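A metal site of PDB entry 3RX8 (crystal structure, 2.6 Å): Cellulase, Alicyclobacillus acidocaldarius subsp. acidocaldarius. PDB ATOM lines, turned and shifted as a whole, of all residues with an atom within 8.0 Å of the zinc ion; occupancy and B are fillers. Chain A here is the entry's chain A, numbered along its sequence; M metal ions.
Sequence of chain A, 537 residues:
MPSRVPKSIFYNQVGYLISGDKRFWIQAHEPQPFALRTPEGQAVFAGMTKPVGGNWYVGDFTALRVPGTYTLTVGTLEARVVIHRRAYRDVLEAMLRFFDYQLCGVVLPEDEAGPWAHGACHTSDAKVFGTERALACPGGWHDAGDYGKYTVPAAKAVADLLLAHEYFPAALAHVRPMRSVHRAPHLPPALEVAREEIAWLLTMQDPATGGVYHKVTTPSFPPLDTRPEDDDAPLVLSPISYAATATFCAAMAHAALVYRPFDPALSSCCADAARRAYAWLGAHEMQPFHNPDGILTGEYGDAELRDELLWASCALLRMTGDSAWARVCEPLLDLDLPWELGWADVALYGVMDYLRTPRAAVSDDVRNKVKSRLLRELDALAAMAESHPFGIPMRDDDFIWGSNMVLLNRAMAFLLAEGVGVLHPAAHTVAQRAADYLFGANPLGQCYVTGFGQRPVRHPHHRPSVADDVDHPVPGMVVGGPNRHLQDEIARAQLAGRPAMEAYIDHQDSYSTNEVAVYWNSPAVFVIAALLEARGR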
ATOM      1  N   GLN A 102     -19.174  24.191  23.488  1.00  0.00           N
ATOM      2  CA  GLN A 102     -18.614  22.923  23.043  1.00  0.00           C
ATOM      3  C   GLN A 102     -19.647  22.002  22.447  1.00  0.00           C
ATOM      4  O   GLN A 102     -19.284  20.896  22.066  1.00  0.00           O
ATOM      5  CB  GLN A 102     -17.887  22.184  24.206  1.00  0.00           C
ATOM      6  CG  GLN A 102     -16.637  22.866  24.723  1.00  0.00           C
ATOM      7  CD  GLN A 102     -15.525  22.918  23.704  1.00  0.00           C
ATOM      8  OE1 GLN A 102     -15.398  23.882  22.956  1.00  0.00           O
ATOM      9  NE2 GLN A 102     -14.678  21.909  23.659  1.00  0.00           N
ATOM     10  N   LEU A 103     -20.936  22.450  22.353  1.00  0.00           N
ATOM     11  CA  LEU A 103     -21.953  21.564  21.798  1.00  0.00           C
ATOM     12  C   LEU A 103     -21.722  21.111  20.340  1.00  0.00           C
ATOM     13  O   LEU A 103     -21.378  21.925  19.488  1.00  0.00           O
ATOM     14  CB  LEU A 103     -23.385  22.103  22.022  1.00  0.00           C
ATOM     15  CG  LEU A 103     -23.927  21.950  23.442  1.00  0.00           C
ATOM     16  CD1 LEU A 103     -25.090  22.887  23.686  1.00  0.00           C
ATOM     17  CD2 LEU A 103     -24.308  20.516  23.738  1.00  0.00           C
ATOM     18  N   CYS A 104     -21.883  19.795  20.083  1.00  0.00           N
ATOM     19  CA  CYS A 104     -21.779  19.127  18.772  1.00  0.00           C
ATOM     20  C   CYS A 104     -23.173  18.850  18.210  1.00  0.00           C
ATOM     21  O   CYS A 104     -24.046  18.391  18.945  1.00  0.00           O
ATOM     22  CB  CYS A 104     -20.974  17.835  18.907  1.00  0.00           C
ATOM     23  SG  CYS A 104     -20.514  17.073  17.325  1.00  0.00           S
ATOM     24  N   GLY A 105     -23.344  19.117  16.905  1.00  0.00           N
ATOM     25  CA  GLY A 105     -24.587  18.875  16.152  1.00  0.00           C
ATOM     26  C   GLY A 105     -25.806  19.696  16.514  1.00  0.00           C
ATOM     27  O   GLY A 105     -26.930  19.306  16.220  1.00  0.00           O
ATOM     28  N   VAL A 106     -25.578  20.832  17.182  1.00  0.00           N
ATOM     29  CA  VAL A 106     -26.600  21.731  17.697  1.00  0.00           C
ATOM     30  C   VAL A 106     -26.315  23.109  17.073  1.00  0.00           C
ATOM     31  O   VAL A 106     -25.150  23.525  17.043  1.00  0.00           O
ATOM     32  CB  VAL A 106     -26.531  21.818  19.256  1.00  0.00           C
ATOM     33  CG1 VAL A 106     -27.688  22.615  19.830  1.00  0.00           C
ATOM     34  CG2 VAL A 106     -26.479  20.444  19.898  1.00  0.00           C
ATOM     35  N   HIS A 118     -22.411  29.240  15.530  1.00  0.00           N
ATOM     36  CA  HIS A 118     -22.214  28.376  14.367  1.00  0.00           C
ATOM     37  C   HIS A 118     -23.355  27.387  14.145  1.00  0.00           C
ATOM     38  O   HIS A 118     -24.139  27.101  15.051  1.00  0.00           O
ATOM     39  CB  HIS A 118     -20.866  27.655  14.446  1.00  0.00           C
ATOM     40  CG  HIS A 118     -20.729  26.702  15.584  1.00  0.00           C
ATOM     41  ND1 HIS A 118     -21.315  25.435  15.558  1.00  0.00           N
ATOM     42  CD2 HIS A 118     -20.004  26.827  16.729  1.00  0.00           C
ATOM     43  CE1 HIS A 118     -20.962  24.848  16.690  1.00  0.00           C
ATOM     44  NE2 HIS A 118     -20.164  25.640  17.422  1.00  0.00           N
ATOM     45  N   GLY A 119     -23.386  26.829  12.938  1.00  0.00           N
ATOM     46  CA  GLY A 119     -24.373  25.821  12.541  1.00  0.00           C
ATOM     47  C   GLY A 119     -24.006  24.452  13.058  1.00  0.00           C
ATOM     48  O   GLY A 119     -22.923  24.262  13.600  1.00  0.00           O
ATOM     49  N   ALA A 120     -24.931  23.493  12.920  1.00  0.00           N
ATOM     50  CA  ALA A 120     -24.785  22.110  13.358  1.00  0.00           C
ATOM     51  C   ALA A 120     -23.615  21.397  12.690  1.00  0.00           C
ATOM     52  O   ALA A 120     -23.598  21.235  11.465  1.00  0.00           O
ATOM     53  CB  ALA A 120     -26.072  21.349  13.115  1.00  0.00           C
ATOM     54  N   CYS A 121     -22.633  21.001  13.512  1.00  0.00           N
ATOM     55  CA  CYS A 121     -21.416  20.325  13.088  1.00  0.00           C
ATOM     56  C   CYS A 121     -21.470  18.853  13.387  1.00  0.00           C
ATOM     57  O   CYS A 121     -22.177  18.455  14.300  1.00  0.00           O
ATOM     58  CB  CYS A 121     -20.205  20.979  13.741  1.00  0.00           C
ATOM     59  SG  CYS A 121     -20.158  20.826  15.545  1.00  0.00           S
ATOM     60  N   HIS A 122     -20.708  18.044  12.627  1.00  0.00           N
ATOM     61  CA  HIS A 122     -20.564  16.594  12.758  1.00  0.00           C
ATOM     62  C   HIS A 122     -21.894  15.791  12.709  1.00  0.00           C
ATOM     63  O   HIS A 122     -22.061  14.798  13.415  1.00  0.00           O
ATOM     64  CB  HIS A 122     -19.693  16.244  13.991  1.00  0.00           C
ATOM     65  CG  HIS A 122     -18.362  16.924  13.972  1.00  0.00           C
ATOM     66  ND1 HIS A 122     -18.117  18.054  14.739  1.00  0.00           N
ATOM     67  CD2 HIS A 122     -17.267  16.655  13.222  1.00  0.00           C
ATOM     68  CE1 HIS A 122     -16.880  18.418  14.440  1.00  0.00           C
ATOM     69  NE2 HIS A 122     -16.320  17.597  13.553  1.00  0.00           N
ATOM     70  N   THR A 123     -22.808  16.238  11.846  1.00  0.00           N
ATOM     71  CA  THR A 123     -24.163  15.681  11.632  1.00  0.00           C
ATOM     72  C   THR A 123     -24.169  14.224  11.109  1.00  0.00           C
ATOM     73  O   THR A 123     -24.963  13.415  11.590  1.00  0.00           O
ATOM     74  CB  THR A 123     -24.998  16.637  10.780  1.00  0.00           C
ATOM     75  OG1 THR A 123     -24.258  16.963   9.588  1.00  0.00           O
ATOM     76  CG2 THR A 123     -25.345  17.923  11.523  1.00  0.00           C
ATOM     77  N   GLY A 139     -24.762  14.998  19.248  1.00  0.00           N
ATOM     78  CA  GLY A 139     -24.842  15.780  20.461  1.00  0.00           C
ATOM     79  C   GLY A 139     -23.559  15.686  21.241  1.00  0.00           C
ATOM     80  O   GLY A 139     -22.516  15.370  20.671  1.00  0.00           O
ATOM     81  N   GLY A 140     -23.637  15.943  22.526  1.00  0.00           N
ATOM     82  CA  GLY A 140     -22.472  15.909  23.386  1.00  0.00           C
ATOM     83  C   GLY A 140     -21.581  17.117  23.221  1.00  0.00           C
ATOM     84  O   GLY A 140     -21.981  18.137  22.625  1.00  0.00           O
ATOM     85  N   TRP A 141     -20.381  17.013  23.756  1.00  0.00           N
ATOM     86  CA  TRP A 141     -19.431  18.114  23.745  1.00  0.00           C
ATOM     87  C   TRP A 141     -18.190  17.747  22.959  1.00  0.00           C
ATOM     88  O   TRP A 141     -17.764  16.605  22.972  1.00  0.00           O
ATOM     89  CB  TRP A 141     -19.005  18.502  25.197  1.00  0.00           C
ATOM     90  CG  TRP A 141     -20.121  18.838  26.133  1.00  0.00           C
ATOM     91  CD1 TRP A 141     -21.213  19.614  25.857  1.00  0.00           C
ATOM     92  CD2 TRP A 141     -20.219  18.508  27.532  1.00  0.00           C
ATOM     93  NE1 TRP A 141     -21.981  19.770  26.988  1.00  0.00           N
ATOM     94  CE2 TRP A 141     -21.396  19.097  28.029  1.00  0.00           C
ATOM     95  CE3 TRP A 141     -19.389  17.807  28.426  1.00  0.00           C
ATOM     96  CZ2 TRP A 141     -21.797  18.981  29.365  1.00  0.00           C
ATOM     97  CZ3 TRP A 141     -19.798  17.659  29.756  1.00  0.00           C
ATOM     98  CH2 TRP A 141     -20.984  18.258  30.213  1.00  0.00           C
ATOM     99  N   HIS A 142     -17.579  18.758  22.324  1.00  0.00           N
ATOM    100  CA  HIS A 142     -16.265  18.617  21.689  1.00  0.00           C
ATOM    101  C   HIS A 142     -15.396  18.586  22.926  1.00  0.00           C
ATOM    102  O   HIS A 142     -15.595  19.404  23.832  1.00  0.00           O
ATOM    103  CB  HIS A 142     -15.929  19.807  20.790  1.00  0.00           C
ATOM    104  CG  HIS A 142     -16.759  19.860  19.542  1.00  0.00           C
ATOM    105  ND1 HIS A 142     -17.244  21.054  19.032  1.00  0.00           N
ATOM    106  CD2 HIS A 142     -17.182  18.845  18.748  1.00  0.00           C
ATOM    107  CE1 HIS A 142     -17.934  20.733  17.964  1.00  0.00           C
ATOM    108  NE2 HIS A 142     -17.909  19.423  17.740  1.00  0.00           N
ATOM    109  N   ASP A 146      -9.853  20.078  20.151  1.00  0.00           N
ATOM    110  CA  ASP A 146     -10.203  19.217  19.034  1.00  0.00           C
ATOM    111  C   ASP A 146     -11.731  18.991  19.107  1.00  0.00           C
ATOM    112  O   ASP A 146     -12.371  19.386  20.095  1.00  0.00           O
ATOM    113  CB  ASP A 146      -9.411  17.888  19.117  1.00  0.00           C
ATOM    114  CG  ASP A 146      -9.789  16.942  20.258  1.00  0.00           C
ATOM    115  OD1 ASP A 146     -10.267  17.436  21.299  1.00  0.00           O
ATOM    116  OD2 ASP A 146      -9.612  15.726  20.095  1.00  0.00           O
ATOM    117  N   TYR A 147     -12.293  18.314  18.086  1.00  0.00           N
ATOM    118  CA  TYR A 147     -13.721  18.050  17.931  1.00  0.00           C
ATOM    119  C   TYR A 147     -14.153  16.638  18.312  1.00  0.00           C
ATOM    120  O   TYR A 147     -15.343  16.300  18.210  1.00  0.00           O
ATOM    121  CB  TYR A 147     -14.182  18.434  16.528  1.00  0.00           C
ATOM    122  CG  TYR A 147     -13.994  19.905  16.219  1.00  0.00           C
ATOM    123  CD1 TYR A 147     -14.546  20.889  17.033  1.00  0.00           C
ATOM    124  CD2 TYR A 147     -13.268  20.313  15.111  1.00  0.00           C
ATOM    125  CE1 TYR A 147     -14.390  22.244  16.741  1.00  0.00           C
ATOM    126  CE2 TYR A 147     -13.089  21.663  14.819  1.00  0.00           C
ATOM    127  CZ  TYR A 147     -13.647  22.626  15.636  1.00  0.00           C
ATOM    128  OH  TYR A 147     -13.493  23.956  15.361  1.00  0.00           O
ATOM    129  N   GLY A 148     -13.205  15.871  18.803  1.00  0.00           N
ATOM    130  CA  GLY A 148     -13.439  14.502  19.267  1.00  0.00           C
ATOM    131  C   GLY A 148     -14.395  14.408  20.441  1.00  0.00           C
ATOM    132  O   GLY A 148     -14.559  15.347  21.219  1.00  0.00           O
ATOM    133  N   LYS A 149     -15.084  13.264  20.530  1.00  0.00           N
ATOM    134  CA  LYS A 149     -16.003  13.044  21.641  1.00  0.00           C
ATOM    135  C   LYS A 149     -15.560  11.757  22.325  1.00  0.00           C
ATOM    136  O   LYS A 149     -15.704  10.676  21.756  1.00  0.00           O
ATOM    137  CB  LYS A 149     -17.445  13.003  21.141  1.00  0.00           C
ATOM    138  CG  LYS A 149     -17.919  14.344  20.575  1.00  0.00           C
ATOM    139  CD  LYS A 149     -19.421  14.422  20.343  1.00  0.00           C
ATOM    140  CE  LYS A 149     -19.896  13.626  19.145  1.00  0.00           C
ATOM    141  NZ  LYS A 149     -21.346  13.735  18.961  1.00  0.00           N
ATOM    142  N   PRO A 228     -15.987  24.465  13.287  1.00  0.00           N
ATOM    143  CA  PRO A 228     -16.676  23.181  13.580  1.00  0.00           C
ATOM    144  C   PRO A 228     -17.434  22.553  12.386  1.00  0.00           C
ATOM    145  O   PRO A 228     -17.308  21.330  12.159  1.00  0.00           O
ATOM    146  CB  PRO A 228     -17.587  23.481  14.781  1.00  0.00           C
ATOM    147  CG  PRO A 228     -17.346  24.893  15.147  1.00  0.00           C
ATOM    148  CD  PRO A 228     -16.282  25.503  14.307  1.00  0.00           C
ATOM    149  N   GLU A 229     -18.176  23.381  11.607  1.00  0.00           N
ATOM    150  CA  GLU A 229     -18.976  22.910  10.454  1.00  0.00           C
ATOM    151  C   GLU A 229     -18.217  22.619   9.165  1.00  0.00           C
ATOM    152  O   GLU A 229     -18.751  21.964   8.262  1.00  0.00           O
ATOM    153  CB  GLU A 229     -20.253  23.724  10.246  1.00  0.00           C
ATOM    154  CG  GLU A 229     -20.015  25.171   9.897  1.00  0.00           C
ATOM    155  CD  GLU A 229     -20.081  26.109  11.086  1.00  0.00           C
ATOM    156  OE1 GLU A 229     -19.146  26.077  11.926  1.00  0.00           O
ATOM    157  OE2 GLU A 229     -21.070  26.870  11.170  1.00  0.00           O
ATOM    158  N   ASP A 231     -15.372  20.820   9.336  1.00  0.00           N
ATOM    159  CA  ASP A 231     -14.685  19.559   9.625  1.00  0.00           C
ATOM    160  C   ASP A 231     -15.570  18.428   9.113  1.00  0.00           C
ATOM    161  O   ASP A 231     -16.542  18.024   9.780  1.00  0.00           O
ATOM    162  CB  ASP A 231     -14.352  19.433  11.129  1.00  0.00           C
ATOM    163  CG  ASP A 231     -13.611  18.161  11.522  1.00  0.00           C
ATOM    164  OD1 ASP A 231     -13.054  17.483  10.618  1.00  0.00           O
ATOM    165  OD2 ASP A 231     -13.561  17.854  12.742  1.00  0.00           O
ATOM    166  N   LEU A 235     -16.476  10.040  10.387  1.00  0.00           N
ATOM    167  CA  LEU A 235     -16.444   9.834  11.830  1.00  0.00           C
ATOM    168  C   LEU A 235     -16.366   8.342  12.033  1.00  0.00           C
ATOM    169  O   LEU A 235     -17.022   7.580  11.297  1.00  0.00           O
ATOM    170  CB  LEU A 235     -17.718  10.399  12.493  1.00  0.00           C
ATOM    171  CG  LEU A 235     -17.980  11.915  12.384  1.00  0.00           C
ATOM    172  CD1 LEU A 235     -19.386  12.252  12.873  1.00  0.00           C
ATOM    173  CD2 LEU A 235     -16.988  12.716  13.185  1.00  0.00           C
HETATM  174 ZN    ZN M   1     -19.290  18.809  16.345  1.00  0.00          ZN
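O of His 142 is in hydrogen-bond range of NE2 of Gln 102 (2.7 Å).
NE2 of His 122 is in hydrogen-bond range of OD2 of Asp 231 (2.9 Å).
O of Cys 121 is in hydrogen-bond range of N of Gly 105 (2.9 Å).
The backbone NH of Gly 139 lies close to the backbone carbonyl oxygen of Cys 104, at 3.5 Å.
N of Cys 104 is in hydrogen-bond range of O of Gly 140, at 3.0 Å.
The zinc ion is bound by NE2 of His 142, ND1 of His 122, SG of Cys 121 and SG of Cys 104.
Within 4 Å of the zinc ion: Cys 104, Cys 121, His 122 and His 142.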
